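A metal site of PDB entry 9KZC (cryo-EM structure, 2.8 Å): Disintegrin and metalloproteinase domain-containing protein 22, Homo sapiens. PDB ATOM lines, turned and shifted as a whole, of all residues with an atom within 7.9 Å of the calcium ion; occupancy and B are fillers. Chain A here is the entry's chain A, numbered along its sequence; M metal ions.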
ATOM      1  N   ALA A 200      -7.743  10.240  30.224  1.00  0.00           N
ATOM      2  CA  ALA A 200      -8.973  10.539  29.501  1.00  0.00           C
ATOM      3  C   ALA A 200      -9.371   9.436  28.534  1.00  0.00           C
ATOM      4  O   ALA A 200     -10.498   9.460  28.023  1.00  0.00           O
ATOM      5  CB  ALA A 200      -8.834  11.863  28.756  1.00  0.00           C
ATOM      6  N   PHE A 203     -12.290   6.004  29.597  1.00  0.00           N
ATOM      7  CA  PHE A 203     -13.722   6.168  29.774  1.00  0.00           C
ATOM      8  C   PHE A 203     -14.546   5.560  28.641  1.00  0.00           C
ATOM      9  O   PHE A 203     -15.750   5.785  28.578  1.00  0.00           O
ATOM     10  CB  PHE A 203     -14.065   7.648  29.939  1.00  0.00           C
ATOM     11  CG  PHE A 203     -13.493   8.253  31.186  1.00  0.00           C
ATOM     12  CD1 PHE A 203     -14.166   8.153  32.389  1.00  0.00           C
ATOM     13  CD2 PHE A 203     -12.260   8.894  31.152  1.00  0.00           C
ATOM     14  CE1 PHE A 203     -13.628   8.700  33.536  1.00  0.00           C
ATOM     15  CE2 PHE A 203     -11.728   9.433  32.309  1.00  0.00           C
ATOM     16  CZ  PHE A 203     -12.409   9.338  33.489  1.00  0.00           C
ATOM     17  N   ARG A 272     -20.822  13.763  31.782  1.00  0.00           N
ATOM     18  CA  ARG A 272     -19.508  13.927  32.386  1.00  0.00           C
ATOM     19  C   ARG A 272     -19.169  15.416  32.395  1.00  0.00           C
ATOM     20  O   ARG A 272     -18.933  15.994  31.334  1.00  0.00           O
ATOM     21  CB  ARG A 272     -18.436  13.132  31.630  1.00  0.00           C
ATOM     22  CG  ARG A 272     -17.160  12.903  32.419  1.00  0.00           C
ATOM     23  CD  ARG A 272     -16.220  11.977  31.661  1.00  0.00           C
ATOM     24  NE  ARG A 272     -16.822  10.676  31.412  1.00  0.00           N
ATOM     25  CZ  ARG A 272     -17.077  10.189  30.207  1.00  0.00           C
ATOM     26  NH1 ARG A 272     -16.796  10.871  29.115  1.00  0.00           N
ATOM     27  NH2 ARG A 272     -17.621   8.978  30.099  1.00  0.00           N
ATOM     28  N   GLU A 273     -19.151  16.009  33.581  1.00  0.00           N
ATOM     29  CA  GLU A 273     -18.770  17.404  33.702  1.00  0.00           C
ATOM     30  C   GLU A 273     -17.252  17.544  33.614  1.00  0.00           C
ATOM     31  O   GLU A 273     -16.512  16.618  33.945  1.00  0.00           O
ATOM     32  CB  GLU A 273     -19.272  17.980  35.032  1.00  0.00           C
ATOM     33  CG  GLU A 273     -19.220  19.492  35.128  1.00  0.00           C
ATOM     34  CD  GLU A 273     -20.008  20.181  34.028  1.00  0.00           C
ATOM     35  OE1 GLU A 273     -21.224  19.938  33.927  1.00  0.00           O
ATOM     36  OE2 GLU A 273     -19.401  20.966  33.260  1.00  0.00           O
ATOM     37  N   ALA A 274     -16.813  18.711  33.150  1.00  0.00           N
ATOM     38  CA  ALA A 274     -15.376  18.973  33.045  1.00  0.00           C
ATOM     39  C   ALA A 274     -14.726  18.904  34.419  1.00  0.00           C
ATOM     40  O   ALA A 274     -15.204  19.501  35.382  1.00  0.00           O
ATOM     41  CB  ALA A 274     -15.140  20.346  32.408  1.00  0.00           C
ATOM     42  N   VAL A 275     -13.611  18.167  34.497  1.00  0.00           N
ATOM     43  CA  VAL A 275     -12.939  18.010  35.777  1.00  0.00           C
ATOM     44  C   VAL A 275     -11.988  19.172  36.051  1.00  0.00           C
ATOM     45  O   VAL A 275     -11.726  19.501  37.211  1.00  0.00           O
ATOM     46  CB  VAL A 275     -12.195  16.663  35.829  1.00  0.00           C
ATOM     47  CG1 VAL A 275     -13.181  15.509  35.805  1.00  0.00           C
ATOM     48  CG2 VAL A 275     -11.209  16.550  34.680  1.00  0.00           C
ATOM     49  N   ASN A 276     -11.473  19.820  35.009  1.00  0.00           N
ATOM     50  CA  ASN A 276     -10.584  20.950  35.162  1.00  0.00           C
ATOM     51  C   ASN A 276     -10.784  21.891  33.981  1.00  0.00           C
ATOM     52  O   ASN A 276     -11.761  21.780  33.230  1.00  0.00           O
ATOM     53  CB  ASN A 276      -9.131  20.483  35.312  1.00  0.00           C
ATOM     54  CG  ASN A 276      -8.631  19.730  34.091  1.00  0.00           C
ATOM     55  OD1 ASN A 276      -9.394  19.035  33.429  1.00  0.00           O
ATOM     56  ND2 ASN A 276      -7.340  19.880  33.796  1.00  0.00           N
ATOM     57  N   CYS A 278      -8.918  22.261  31.240  1.00  0.00           N
ATOM     58  CA  CYS A 278      -8.606  21.689  29.939  1.00  0.00           C
ATOM     59  C   CYS A 278      -9.650  20.688  29.456  1.00  0.00           C
ATOM     60  O   CYS A 278      -9.575  20.250  28.311  1.00  0.00           O
ATOM     61  CB  CYS A 278      -7.236  21.012  29.961  1.00  0.00           C
ATOM     62  SG  CYS A 278      -5.858  22.111  30.351  1.00  0.00           S
ATOM     63  N   ASP A 279     -10.607  20.309  30.301  1.00  0.00           N
ATOM     64  CA  ASP A 279     -11.577  19.289  29.937  1.00  0.00           C
ATOM     65  C   ASP A 279     -12.793  19.905  29.272  1.00  0.00           C
ATOM     66  O   ASP A 279     -13.152  21.056  29.523  1.00  0.00           O
ATOM     67  CB  ASP A 279     -12.006  18.496  31.177  1.00  0.00           C
ATOM     68  CG  ASP A 279     -12.716  17.214  30.831  1.00  0.00           C
ATOM     69  OD1 ASP A 279     -12.572  16.750  29.677  1.00  0.00           O
ATOM     70  OD2 ASP A 279     -13.410  16.648  31.703  1.00  0.00           O
ATOM     71  N   ILE A 280     -13.430  19.117  28.402  1.00  0.00           N
ATOM     72  CA  ILE A 280     -14.628  19.519  27.679  1.00  0.00           C
ATOM     73  C   ILE A 280     -15.797  18.688  28.189  1.00  0.00           C
ATOM     74  O   ILE A 280     -15.691  17.455  28.288  1.00  0.00           O
ATOM     75  CB  ILE A 280     -14.449  19.355  26.152  1.00  0.00           C
ATOM     76  CG1 ILE A 280     -13.652  20.521  25.578  1.00  0.00           C
ATOM     77  CG2 ILE A 280     -15.792  19.240  25.462  1.00  0.00           C
ATOM     78  CD1 ILE A 280     -12.969  20.197  24.273  1.00  0.00           C
ATOM     79  N   ARG A 281     -16.887  19.354  28.527  1.00  0.00           N
ATOM     80  CA  ARG A 281     -18.080  18.659  29.000  1.00  0.00           C
ATOM     81  C   ARG A 281     -18.623  17.743  27.905  1.00  0.00           C
ATOM     82  O   ARG A 281     -18.661  18.100  26.734  1.00  0.00           O
ATOM     83  CB  ARG A 281     -19.147  19.671  29.423  1.00  0.00           C
ATOM     84  CG  ARG A 281     -20.420  19.059  29.964  1.00  0.00           C
ATOM     85  CD  ARG A 281     -21.279  20.117  30.645  1.00  0.00           C
ATOM     86  NE  ARG A 281     -21.775  21.100  29.692  1.00  0.00           N
ATOM     87  CZ  ARG A 281     -22.833  20.921  28.913  1.00  0.00           C
ATOM     88  NH1 ARG A 281     -23.533  19.795  28.942  1.00  0.00           N
ATOM     89  NH2 ARG A 281     -23.185  21.890  28.075  1.00  0.00           N
ATOM     90  N   GLU A 282     -19.052  16.547  28.303  1.00  0.00           N
ATOM     91  CA  GLU A 282     -19.599  15.559  27.397  1.00  0.00           C
ATOM     92  C   GLU A 282     -21.112  15.506  27.535  1.00  0.00           C
ATOM     93  O   GLU A 282     -21.631  15.420  28.654  1.00  0.00           O
ATOM     94  CB  GLU A 282     -18.999  14.169  27.651  1.00  0.00           C
ATOM     95  CG  GLU A 282     -17.679  13.920  26.938  1.00  0.00           C
ATOM     96  CD  GLU A 282     -16.476  14.344  27.753  1.00  0.00           C
ATOM     97  OE1 GLU A 282     -16.501  14.132  28.989  1.00  0.00           O
ATOM     98  OE2 GLU A 282     -15.518  14.881  27.172  1.00  0.00           O
ATOM     99  N   THR A 283     -21.818  15.553  26.413  1.00  0.00           N
ATOM    100  CA  THR A 283     -23.264  15.532  26.377  1.00  0.00           C
ATOM    101  C   THR A 283     -23.758  14.257  25.712  1.00  0.00           C
ATOM    102  O   THR A 283     -23.128  13.730  24.789  1.00  0.00           O
ATOM    103  CB  THR A 283     -23.823  16.752  25.633  1.00  0.00           C
ATOM    104  OG1 THR A 283     -23.561  16.620  24.232  1.00  0.00           O
ATOM    105  CG2 THR A 283     -23.164  18.030  26.143  1.00  0.00           C
ATOM    106  N   CYS A 291     -22.008   7.195  27.603  1.00  0.00           N
ATOM    107  CA  CYS A 291     -21.625   8.577  27.346  1.00  0.00           C
ATOM    108  C   CYS A 291     -20.493   8.646  26.338  1.00  0.00           C
ATOM    109  O   CYS A 291     -19.743   7.674  26.137  1.00  0.00           O
ATOM    110  CB  CYS A 291     -21.218   9.265  28.650  1.00  0.00           C
ATOM    111  SG  CYS A 291     -20.538  10.938  28.461  1.00  0.00           S
ATOM    112  N   ALA A 292     -20.365   9.797  25.679  1.00  0.00           N
ATOM    113  CA  ALA A 292     -19.358   9.967  24.648  1.00  0.00           C
ATOM    114  C   ALA A 292     -17.963   9.846  25.247  1.00  0.00           C
ATOM    115  O   ALA A 292     -17.760  10.101  26.431  1.00  0.00           O
ATOM    116  CB  ALA A 292     -19.527  11.328  23.965  1.00  0.00           C
ATOM    117  N   PRO A 293     -16.978   9.418  24.451  1.00  0.00           N
ATOM    118  CA  PRO A 293     -15.607   9.287  24.974  1.00  0.00           C
ATOM    119  C   PRO A 293     -15.080  10.614  25.498  1.00  0.00           C
ATOM    120  O   PRO A 293     -15.382  11.682  24.976  1.00  0.00           O
ATOM    121  CB  PRO A 293     -14.807   8.798  23.761  1.00  0.00           C
ATOM    122  CG  PRO A 293     -15.646   9.152  22.573  1.00  0.00           C
ATOM    123  CD  PRO A 293     -17.060   9.001  23.035  1.00  0.00           C
ATOM    124  N   ASN A 294     -14.278  10.525  26.555  1.00  0.00           N
ATOM    125  CA  ASN A 294     -13.780  11.706  27.254  1.00  0.00           C
ATOM    126  C   ASN A 294     -12.796  12.446  26.365  1.00  0.00           C
ATOM    127  O   ASN A 294     -11.657  12.020  26.186  1.00  0.00           O
ATOM    128  CB  ASN A 294     -13.136  11.303  28.581  1.00  0.00           C
ATOM    129  CG  ASN A 294     -12.873  12.474  29.484  1.00  0.00           C
ATOM    130  OD1 ASN A 294     -13.075  13.630  29.102  1.00  0.00           O
ATOM    131  ND2 ASN A 294     -12.413  12.199  30.695  1.00  0.00           N
ATOM    132  N   ILE A 295     -13.247  13.557  25.801  1.00  0.00           N
ATOM    133  CA  ILE A 295     -12.404  14.442  25.003  1.00  0.00           C
ATOM    134  C   ILE A 295     -12.098  15.683  25.825  1.00  0.00           C
ATOM    135  O   ILE A 295     -12.904  16.118  26.663  1.00  0.00           O
ATOM    136  CB  ILE A 295     -13.063  14.809  23.656  1.00  0.00           C
ATOM    137  CG1 ILE A 295     -14.410  15.496  23.895  1.00  0.00           C
ATOM    138  CG2 ILE A 295     -13.243  13.574  22.797  1.00  0.00           C
ATOM    139  CD1 ILE A 295     -15.053  16.034  22.640  1.00  0.00           C
ATOM    140  N   HIS A 296     -10.923  16.257  25.585  1.00  0.00           N
ATOM    141  CA  HIS A 296     -10.529  17.488  26.267  1.00  0.00           C
ATOM    142  C   HIS A 296     -10.007  18.496  25.249  1.00  0.00           C
ATOM    143  O   HIS A 296     -10.041  18.231  24.046  1.00  0.00           O
ATOM    144  CB  HIS A 296      -9.479  17.208  27.337  1.00  0.00           C
ATOM    145  CG  HIS A 296      -8.440  16.217  26.909  1.00  0.00           C
ATOM    146  ND1 HIS A 296      -7.339  16.575  26.152  1.00  0.00           N
ATOM    147  CD2 HIS A 296      -8.326  14.887  27.145  1.00  0.00           C
ATOM    148  CE1 HIS A 296      -6.600  15.494  25.932  1.00  0.00           C
ATOM    149  NE2 HIS A 296      -7.172  14.471  26.522  1.00  0.00           N
ATOM    150  N   LYS A 297      -9.525  19.643  25.716  1.00  0.00           N
ATOM    151  CA  LYS A 297      -8.964  20.630  24.813  1.00  0.00           C
ATOM    152  C   LYS A 297      -7.634  20.153  24.250  1.00  0.00           C
ATOM    153  O   LYS A 297      -6.913  19.380  24.900  1.00  0.00           O
ATOM    154  CB  LYS A 297      -8.785  21.972  25.539  1.00  0.00           C
ATOM    155  CG  LYS A 297     -10.092  22.595  25.993  1.00  0.00           C
ATOM    156  CD  LYS A 297      -9.872  23.918  26.693  1.00  0.00           C
ATOM    157  CE  LYS A 297     -11.187  24.514  27.162  1.00  0.00           C
ATOM    158  NZ  LYS A 297     -11.003  25.829  27.829  1.00  0.00           N
HETATM  159 CA    CA M   1     -14.615  15.549  29.416  1.00  0.00          CA
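Merely in contact with the calcium ion: Ile 295 (3.3 Å).
The side-chain carboxylate of Asp 279 lies close to the backbone NH of Val 275, at 3.2 Å.
The side-chain carboxylate (OE2) of Glu 282 lies close to the backbone NH (N) of Ile 295, at 3.0 Å.
The backbone carbonyl oxygen (O) of Arg 272 is in hydrogen-bond range of the backbone NH (N) of Glu 282, at 3.1 Å.
The calcium ion is bound by OD1 of Asp 279 (2.4 Å), OE1 of Glu 282 (2.4 Å), O of Ile 280 (2.5 Å), OD1 of Asn 294 (2.5 Å), OE2 of Glu 282 (2.5 Å) and OD2 of Asp 279 (2.8 Å).
The calcium ion has six donor atoms within binding distance.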
